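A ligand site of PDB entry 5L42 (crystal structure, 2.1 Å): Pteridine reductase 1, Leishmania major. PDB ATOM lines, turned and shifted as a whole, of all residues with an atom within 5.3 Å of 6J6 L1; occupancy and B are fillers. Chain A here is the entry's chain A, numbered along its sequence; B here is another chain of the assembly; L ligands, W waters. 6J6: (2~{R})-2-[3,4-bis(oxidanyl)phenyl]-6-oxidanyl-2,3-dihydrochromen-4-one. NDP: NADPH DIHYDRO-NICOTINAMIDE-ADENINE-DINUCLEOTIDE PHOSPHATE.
Ser 111 touches 6J6 L1 (OG to OAT, 3.6 Å).
Phe 113 touches 6J6 L1.
Leu 188 touches 6J6 L1 (CD1 to OAH, 3.7 Å).
OH of Tyr 194 touches CAP of 6J6 L1, 3.4 Å away.
Gly 225 touches 6J6 L1 (O to CAB, 3.3 Å).
Leu 226 touches 6J6 L1.
An oxygen (OAT) of 6J6 L1 is in hydrogen-bond range of an oxygen (O1A) of NDP L2 (2.8 Å).
The guanidinium group (NH1) of Arg 17 is in hydrogen-bond range of the backbone carbonyl oxygen (O) of Val 228.
The side-chain hydroxyl of Tyr 194 is in hydrogen-bond range of the side-chain carboxylate of Asp 181 (2.6 Å).
The guanidinium group (NH2) of Arg 287 of chain B sits at hydrogen-bond distance from the backbone carbonyl oxygen (O) of Met 183, at 3.3 Å.
Water W3 lies within hydrogen-bond range of N of Val 230 (2.7 Å) and OAO of 6J6 L1 (2.8 Å).
Water W6 bridges an oxygen (OAG) of 6J6 L1 (2.8 Å) and the side-chain hydroxyl (OH) of Tyr 283 (3.5 Å).
Water W2 bridges NE2 of His 241 and OAH of 6J6 L1.
Water W1 lies within hydrogen-bond range of the side-chain carboxylate (OD1) of Asp 181 (2.8 Å) and the backbone carbonyl oxygen (O) of Gly 225 (2.8 Å).
Water W5 lies within hydrogen-bond range of the side-chain hydroxyl of Tyr 283, the backbone carbonyl oxygen of His 241 and an oxygen (OAG) of 6J6 L1.
The side-chain hydroxyl (OG) of Ser 111 sits at hydrogen-bond distance from an oxygen (O2D) of NDP L2, 2.9 Å away.
NH2 of Arg 17 sits at hydrogen-bond distance from OAO of 6J6 L1 (3.3 Å).
NH2 of Arg 17 lies within salt-bridge range of O1N of NDP L2 (2.8 Å).
N of Ser 227 is in hydrogen-bond range of O7N of NDP L2 (2.7 Å).
The side-chain hydroxyl (OH) of Tyr 283 sits at hydrogen-bond distance from an oxygen (OAG) of 6J6 L1, at 3.4 Å.
A nitrogen (N7A) of NDP L2 sits at hydrogen-bond distance from the side-chain hydroxyl of Ser 112 (2.7 Å).
The backbone carbonyl oxygen of Ser 227 sits at hydrogen-bond distance from a nitrogen (N7N) of NDP L2 (2.9 Å).
O4B of NDP L2 sits at hydrogen-bond distance from N of Ser 111 (3.1 Å).
OAG of 6J6 L1 lies within hydrogen-bond range of NH1 of Arg 287 of chain B, 3.0 Å away.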
ATOM      1  N   ARG A  17      -3.084  28.063   0.015  1.00  0.00           N
ATOM      2  CA  ARG A  17      -2.474  26.729   0.208  1.00  0.00           C
ATOM      3  C   ARG A  17      -1.139  26.795   0.994  1.00  0.00           C
ATOM      4  O   ARG A  17      -1.079  27.493   2.004  1.00  0.00           O
ATOM      5  CB  ARG A  17      -2.364  26.084  -1.179  1.00  0.00           C
ATOM      6  CG  ARG A  17      -3.762  25.764  -1.748  1.00  0.00           C
ATOM      7  CD  ARG A  17      -3.701  25.337  -3.232  1.00  0.00           C
ATOM      8  NE  ARG A  17      -2.788  24.170  -3.401  1.00  0.00           N
ATOM      9  CZ  ARG A  17      -3.125  22.938  -3.013  1.00  0.00           C
ATOM     10  NH1 ARG A  17      -4.354  22.656  -2.512  1.00  0.00           N
ATOM     11  NH2 ARG A  17      -2.223  21.947  -3.127  1.00  0.00           N
ATOM     12  N   SER A 111       4.862  27.687  -8.057  1.00  0.00           N
ATOM     13  CA  SER A 111       5.027  26.468  -8.813  1.00  0.00           C
ATOM     14  C   SER A 111       3.888  26.219  -9.755  1.00  0.00           C
ATOM     15  O   SER A 111       2.745  26.168  -9.324  1.00  0.00           O
ATOM     16  CB  SER A 111       5.062  25.247  -7.871  1.00  0.00           C
ATOM     17  OG  SER A 111       5.212  24.040  -8.639  1.00  0.00           O
ATOM     18  N   SER A 112       4.200  25.957 -11.002  1.00  0.00           N
ATOM     19  CA  SER A 112       3.209  25.444 -11.959  1.00  0.00           C
ATOM     20  C   SER A 112       3.285  23.921 -12.019  1.00  0.00           C
ATOM     21  O   SER A 112       4.392  23.333 -11.916  1.00  0.00           O
ATOM     22  CB  SER A 112       3.471  26.066 -13.319  1.00  0.00           C
ATOM     23  OG  SER A 112       3.433  27.479 -13.223  1.00  0.00           O
ATOM     24  N   PHE A 113       2.142  23.261 -12.184  1.00  0.00           N
ATOM     25  CA  PHE A 113       2.145  21.791 -12.148  1.00  0.00           C
ATOM     26  C   PHE A 113       1.003  21.277 -12.995  1.00  0.00           C
ATOM     27  O   PHE A 113      -0.158  21.507 -12.635  1.00  0.00           O
ATOM     28  CB  PHE A 113       2.001  21.341 -10.693  1.00  0.00           C
ATOM     29  CG  PHE A 113       1.652  19.870 -10.507  1.00  0.00           C
ATOM     30  CD1 PHE A 113       2.629  18.879 -10.589  1.00  0.00           C
ATOM     31  CD2 PHE A 113       0.329  19.490 -10.197  1.00  0.00           C
ATOM     32  CE1 PHE A 113       2.322  17.524 -10.356  1.00  0.00           C
ATOM     33  CE2 PHE A 113      -0.028  18.147 -10.008  1.00  0.00           C
ATOM     34  CZ  PHE A 113       0.994  17.144 -10.087  1.00  0.00           C
ATOM     35  N   ASP A 181      10.050  18.459  -4.320  1.00  0.00           N
ATOM     36  CA  ASP A 181       8.987  17.451  -4.266  1.00  0.00           C
ATOM     37  C   ASP A 181       9.524  16.102  -3.766  1.00  0.00           C
ATOM     38  O   ASP A 181      10.481  15.536  -4.378  1.00  0.00           O
ATOM     39  CB  ASP A 181       8.533  17.356  -5.759  1.00  0.00           C
ATOM     40  CG  ASP A 181       7.312  16.413  -5.970  1.00  0.00           C
ATOM     41  OD1 ASP A 181       7.060  15.462  -5.138  1.00  0.00           O
ATOM     42  OD2 ASP A 181       6.556  16.653  -6.963  1.00  0.00           O
ATOM     43  N   MET A 183       8.579  13.268  -4.225  1.00  0.00           N
ATOM     44  CA  MET A 183       8.141  12.124  -4.977  1.00  0.00           C
ATOM     45  C   MET A 183       8.732  12.065  -6.361  1.00  0.00           C
ATOM     46  O   MET A 183       8.502  11.072  -7.086  1.00  0.00           O
ATOM     47  CB  MET A 183       6.579  12.052  -5.080  1.00  0.00           C
ATOM     48  CG  MET A 183       5.863  11.943  -3.755  1.00  0.00           C
ATOM     49  SD  MET A 183       6.452  10.498  -2.807  1.00  0.00           S
ATOM     50  CE  MET A 183       5.970   9.106  -3.865  1.00  0.00           C
ATOM     51  N   LEU A 188       5.736  11.238 -11.547  1.00  0.00           N
ATOM     52  CA  LEU A 188       4.331  11.142 -11.848  1.00  0.00           C
ATOM     53  C   LEU A 188       4.216  11.041 -13.361  1.00  0.00           C
ATOM     54  O   LEU A 188       4.816  11.823 -14.089  1.00  0.00           O
ATOM     55  CB  LEU A 188       3.656  12.398 -11.250  1.00  0.00           C
ATOM     56  CG  LEU A 188       2.169  12.369 -11.155  1.00  0.00           C
ATOM     57  CD1 LEU A 188       1.754  11.254 -10.171  1.00  0.00           C
ATOM     58  CD2 LEU A 188       1.687  13.745 -10.707  1.00  0.00           C
ATOM     59  N   TYR A 194       7.653  19.176 -15.485  1.00  0.00           N
ATOM     60  CA  TYR A 194       7.565  19.492 -14.078  1.00  0.00           C
ATOM     61  C   TYR A 194       8.633  18.756 -13.268  1.00  0.00           C
ATOM     62  O   TYR A 194       9.325  19.349 -12.422  1.00  0.00           O
ATOM     63  CB  TYR A 194       6.125  19.150 -13.553  1.00  0.00           C
ATOM     64  CG  TYR A 194       6.120  19.122 -11.986  1.00  0.00           C
ATOM     65  CD1 TYR A 194       5.948  20.325 -11.229  1.00  0.00           C
ATOM     66  CD2 TYR A 194       6.308  17.916 -11.291  1.00  0.00           C
ATOM     67  CE1 TYR A 194       5.967  20.301  -9.800  1.00  0.00           C
ATOM     68  CE2 TYR A 194       6.354  17.855  -9.880  1.00  0.00           C
ATOM     69  CZ  TYR A 194       6.189  19.054  -9.160  1.00  0.00           C
ATOM     70  OH  TYR A 194       6.197  19.045  -7.800  1.00  0.00           O
ATOM     71  N   GLY A 225       4.916  15.506  -0.088  1.00  0.00           N
ATOM     72  CA  GLY A 225       4.529  14.369  -0.910  1.00  0.00           C
ATOM     73  C   GLY A 225       3.161  14.677  -1.471  1.00  0.00           C
ATOM     74  O   GLY A 225       2.998  15.092  -2.619  1.00  0.00           O
ATOM     75  N   LEU A 226       2.185  14.455  -0.637  1.00  0.00           N
ATOM     76  CA  LEU A 226       0.764  14.705  -0.958  1.00  0.00           C
ATOM     77  C   LEU A 226       0.320  15.690   0.141  1.00  0.00           C
ATOM     78  O   LEU A 226       0.250  15.332   1.340  1.00  0.00           O
ATOM     79  CB  LEU A 226       0.049  13.349  -0.868  1.00  0.00           C
ATOM     80  CG  LEU A 226      -1.338  13.097  -1.473  1.00  0.00           C
ATOM     81  CD1 LEU A 226      -1.335  13.310  -2.980  1.00  0.00           C
ATOM     82  CD2 LEU A 226      -1.814  11.673  -1.136  1.00  0.00           C
ATOM     83  N   SER A 227       0.084  16.952  -0.241  1.00  0.00           N
ATOM     84  CA  SER A 227      -0.335  17.985   0.721  1.00  0.00           C
ATOM     85  C   SER A 227      -1.521  18.750   0.189  1.00  0.00           C
ATOM     86  O   SER A 227      -1.506  19.145  -0.967  1.00  0.00           O
ATOM     87  CB  SER A 227       0.814  18.971   0.927  1.00  0.00           C
ATOM     88  OG  SER A 227       1.883  18.336   1.576  1.00  0.00           O
ATOM     89  N   VAL A 228      -2.545  18.951   1.051  1.00  0.00           N
ATOM     90  CA  VAL A 228      -3.807  19.634   0.684  1.00  0.00           C
ATOM     91  C   VAL A 228      -4.299  19.238  -0.724  1.00  0.00           C
ATOM     92  O   VAL A 228      -4.513  20.103  -1.651  1.00  0.00           O
ATOM     93  CB  VAL A 228      -3.769  21.154   1.000  1.00  0.00           C
ATOM     94  CG1 VAL A 228      -3.531  21.384   2.486  1.00  0.00           C
ATOM     95  CG2 VAL A 228      -2.679  21.882   0.226  1.00  0.00           C
ATOM     96  N   LEU A 229      -4.500  17.931  -0.896  1.00  0.00           N
ATOM     97  CA  LEU A 229      -4.856  17.386  -2.209  1.00  0.00           C
ATOM     98  C   LEU A 229      -6.203  17.970  -2.696  1.00  0.00           C
ATOM     99  O   LEU A 229      -7.176  17.919  -1.952  1.00  0.00           O
ATOM    100  CB  LEU A 229      -4.877  15.852  -2.143  1.00  0.00           C
ATOM    101  CG  LEU A 229      -5.428  15.155  -3.386  1.00  0.00           C
ATOM    102  CD1 LEU A 229      -4.548  15.310  -4.630  1.00  0.00           C
ATOM    103  CD2 LEU A 229      -5.745  13.686  -3.090  1.00  0.00           C
ATOM    104  N   VAL A 230      -6.259  18.525  -3.897  1.00  0.00           N
ATOM    105  CA  VAL A 230      -7.441  19.336  -4.308  1.00  0.00           C
ATOM    106  C   VAL A 230      -8.590  18.360  -4.578  1.00  0.00           C
ATOM    107  O   VAL A 230      -8.358  17.195  -4.928  1.00  0.00           O
ATOM    108  CB  VAL A 230      -7.188  20.318  -5.510  1.00  0.00           C
ATOM    109  CG1 VAL A 230      -8.471  21.085  -5.901  1.00  0.00           C
ATOM    110  CG2 VAL A 230      -6.114  21.347  -5.172  1.00  0.00           C
ATOM    111  N   HIS A 241      -6.060   8.169  -3.663  1.00  0.00           N
ATOM    112  CA  HIS A 241      -4.775   8.832  -3.515  1.00  0.00           C
ATOM    113  C   HIS A 241      -4.315   8.885  -2.052  1.00  0.00           C
ATOM    114  O   HIS A 241      -3.223   8.436  -1.738  1.00  0.00           O
ATOM    115  CB  HIS A 241      -4.797  10.228  -4.112  1.00  0.00           C
ATOM    116  CG  HIS A 241      -4.779  10.240  -5.596  1.00  0.00           C
ATOM    117  ND1 HIS A 241      -5.883  10.605  -6.338  1.00  0.00           N
ATOM    118  CD2 HIS A 241      -3.827   9.881  -6.481  1.00  0.00           C
ATOM    119  CE1 HIS A 241      -5.589  10.500  -7.623  1.00  0.00           C
ATOM    120  NE2 HIS A 241      -4.353  10.057  -7.739  1.00  0.00           N
ATOM    121  N   TYR A 283       5.392   8.517   2.037  1.00  0.00           N
ATOM    122  CA  TYR A 283       4.946   8.179   0.688  1.00  0.00           C
ATOM    123  C   TYR A 283       6.114   7.694  -0.254  1.00  0.00           C
ATOM    124  O   TYR A 283       5.955   6.756  -1.051  1.00  0.00           O
ATOM    125  CB  TYR A 283       4.091   9.327   0.088  1.00  0.00           C
ATOM    126  CG  TYR A 283       3.285   8.939  -1.175  1.00  0.00           C
ATOM    127  CD1 TYR A 283       2.903   7.604  -1.446  1.00  0.00           C
ATOM    128  CD2 TYR A 283       2.867   9.954  -2.067  1.00  0.00           C
ATOM    129  CE1 TYR A 283       2.184   7.258  -2.591  1.00  0.00           C
ATOM    130  CE2 TYR A 283       2.127   9.623  -3.187  1.00  0.00           C
ATOM    131  CZ  TYR A 283       1.795   8.299  -3.450  1.00  0.00           C
ATOM    132  OH  TYR A 283       1.055   8.056  -4.582  1.00  0.00           O
ATOM    133  N   ARG B 287       5.546   4.369  -7.515  1.00  0.00           N
ATOM    134  CA  ARG B 287       5.088   4.821  -6.197  1.00  0.00           C
ATOM    135  C   ARG B 287       3.752   4.097  -6.019  1.00  0.00           C
ATOM    136  O   ARG B 287       3.125   3.721  -7.047  1.00  0.00           O
ATOM    137  CB  ARG B 287       4.905   6.344  -6.174  1.00  0.00           C
ATOM    138  CG  ARG B 287       3.971   6.882  -7.254  1.00  0.00           C
ATOM    139  CD  ARG B 287       3.613   8.350  -6.990  1.00  0.00           C
ATOM    140  NE  ARG B 287       4.602   9.278  -7.549  1.00  0.00           N
ATOM    141  CZ  ARG B 287       4.480  10.612  -7.537  1.00  0.00           C
ATOM    142  NH1 ARG B 287       3.403  11.191  -6.960  1.00  0.00           N
ATOM    143  NH2 ARG B 287       5.422  11.379  -8.101  1.00  0.00           N
HETATM  144  CAN 6J6 L   1      -0.476  17.408  -5.293  1.00  0.00           C
HETATM  145  CAM 6J6 L   1      -0.363  18.816  -5.508  1.00  0.00           C
HETATM  146  OAO 6J6 L   1      -1.289  19.516  -5.168  1.00  0.00           O
HETATM  147  CAL 6J6 L   1       0.791  19.383  -6.116  1.00  0.00           C
HETATM  148  CAS 6J6 L   1       0.984  20.734  -6.284  1.00  0.00           C
HETATM  149  CAR 6J6 L   1       2.133  21.221  -6.914  1.00  0.00           C
HETATM  150  OAT 6J6 L   1       2.369  22.509  -7.089  1.00  0.00           O
HETATM  151  CAQ 6J6 L   1       3.087  20.359  -7.389  1.00  0.00           C
HETATM  152  CAP 6J6 L   1       2.891  19.016  -7.241  1.00  0.00           C
HETATM  153  CAK 6J6 L   1       1.748  18.531  -6.640  1.00  0.00           C
HETATM  154  OAJ 6J6 L   1       1.573  17.229  -6.501  1.00  0.00           O
HETATM  155  CAI 6J6 L   1       0.287  16.619  -6.385  1.00  0.00           C
HETATM  156  CAC 6J6 L   1       0.374  15.243  -6.250  1.00  0.00           C
HETATM  157  CAD 6J6 L   1      -0.296  14.445  -7.110  1.00  0.00           C
HETATM  158  CAE 6J6 L   1      -0.239  13.073  -7.051  1.00  0.00           C
HETATM  159  OAH 6J6 L   1      -0.932  12.329  -7.921  1.00  0.00           O
HETATM  160  CAF 6J6 L   1       0.539  12.434  -6.082  1.00  0.00           C
HETATM  161  OAG 6J6 L   1       0.595  11.099  -6.043  1.00  0.00           O
HETATM  162  CAA 6J6 L   1       1.253  13.233  -5.192  1.00  0.00           C
HETATM  163  CAB 6J6 L   1       1.150  14.611  -5.288  1.00  0.00           C
HETATM  164  PA  NDP L   2       0.241  25.380  -5.799  1.00  0.00           P
HETATM  165  O1A NDP L   2       0.228  24.272  -6.809  1.00  0.00           O
HETATM  166  O2A NDP L   2      -1.027  25.687  -5.069  1.00  0.00           O
HETATM  167  O5B NDP L   2       0.927  26.708  -6.370  1.00  0.00           O
HETATM  168  C5B NDP L   2       1.349  27.780  -5.539  1.00  0.00           C
HETATM  169  C4B NDP L   2       1.306  29.115  -6.328  1.00  0.00           C
HETATM  170  O4B NDP L   2       2.246  29.175  -7.425  1.00  0.00           O
HETATM  171  C3B NDP L   2       0.000  29.372  -7.069  1.00  0.00           C
HETATM  172  O3B NDP L   2      -0.983  29.766  -6.122  1.00  0.00           O
HETATM  173  C2B NDP L   2       0.383  30.475  -8.085  1.00  0.00           C
HETATM  174  O2B NDP L   2       0.113  31.830  -7.627  1.00  0.00           O
HETATM  175  C1B NDP L   2       1.908  30.337  -8.159  1.00  0.00           C
HETATM  176  N9A NDP L   2       2.325  30.227  -9.538  1.00  0.00           N
HETATM  177  C8A NDP L   2       2.039  29.221 -10.405  1.00  0.00           C
HETATM  178  N7A NDP L   2       2.602  29.532 -11.615  1.00  0.00           N
HETATM  179  C5A NDP L   2       3.201  30.724 -11.509  1.00  0.00           C
HETATM  180  C6A NDP L   2       3.980  31.594 -12.385  1.00  0.00           C
HETATM  181  N6A NDP L   2       4.173  31.243 -13.669  1.00  0.00           N
HETATM  182  N1A NDP L   2       4.466  32.735 -11.846  1.00  0.00           N
HETATM  183  C2A NDP L   2       4.231  33.142 -10.562  1.00  0.00           C
HETATM  184  N3A NDP L   2       3.561  32.369  -9.712  1.00  0.00           N
HETATM  185  C4A NDP L   2       3.039  31.178 -10.127  1.00  0.00           C
HETATM  186  O3  NDP L   2       1.337  24.988  -4.651  1.00  0.00           O
HETATM  187  PN  NDP L   2       1.111  24.106  -3.293  1.00  0.00           P
HETATM  188  O1N NDP L   2       0.399  22.811  -3.587  1.00  0.00           O
HETATM  189  O2N NDP L   2       0.793  24.997  -2.083  1.00  0.00           O
HETATM  190  O5D NDP L   2       2.626  23.612  -3.053  1.00  0.00           O
HETATM  191  C5D NDP L   2       3.631  24.512  -2.574  1.00  0.00           C
HETATM  192  C4D NDP L   2       4.980  24.069  -3.132  1.00  0.00           C
HETATM  193  O4D NDP L   2       5.205  22.684  -2.801  1.00  0.00           O
HETATM  194  C3D NDP L   2       5.131  24.118  -4.638  1.00  0.00           C
HETATM  195  O3D NDP L   2       6.518  24.433  -4.965  1.00  0.00           O
HETATM  196  C2D NDP L   2       4.935  22.686  -5.090  1.00  0.00           C
HETATM  197  O2D NDP L   2       5.567  22.390  -6.306  1.00  0.00           O
HETATM  198  C1D NDP L   2       5.518  21.891  -3.965  1.00  0.00           C
HETATM  199  N1N NDP L   2       4.790  20.634  -3.886  1.00  0.00           N
HETATM  200  C2N NDP L   2       3.517  20.519  -3.448  1.00  0.00           C
HETATM  201  C3N NDP L   2       2.863  19.287  -3.399  1.00  0.00           C
HETATM  202  C7N NDP L   2       1.420  19.153  -2.862  1.00  0.00           C
HETATM  203  O7N NDP L   2       1.031  18.030  -2.551  1.00  0.00           O
HETATM  204  N7N NDP L   2       0.585  20.219  -2.662  1.00  0.00           N
HETATM  205  C4N NDP L   2       3.602  18.035  -3.791  1.00  0.00           C
HETATM  206  C5N NDP L   2       4.980  18.268  -4.261  1.00  0.00           C
HETATM  207  C6N NDP L   2       5.517  19.532  -4.281  1.00  0.00           C
HETATM  208  P2B NDP L   2      -1.285  32.564  -7.998  1.00  0.00           P
HETATM  209  O1X NDP L   2      -1.068  33.895  -7.301  1.00  0.00           O
HETATM  210  O2X NDP L   2      -1.457  32.564  -9.459  1.00  0.00           O
HETATM  211  O3X NDP L   2      -2.332  31.673  -7.425  1.00  0.00           O
HETATM  212  O   HOH W   1       4.395  14.605  -5.029  1.00  0.00           O
HETATM  213  O   HOH W   2      -2.001  10.014  -9.879  1.00  0.00           O
HETATM  214  O   HOH W   3      -3.951  18.774  -5.357  1.00  0.00           O
HETATM  215  O   HOH W   4       3.145  13.877  -7.270  1.00  0.00           O
HETATM  216  O   HOH W   5      -1.620   9.096  -4.400  1.00  0.00           O
HETATM  217  O   HOH W   6      -0.018   8.999  -7.768  1.00  0.00           O
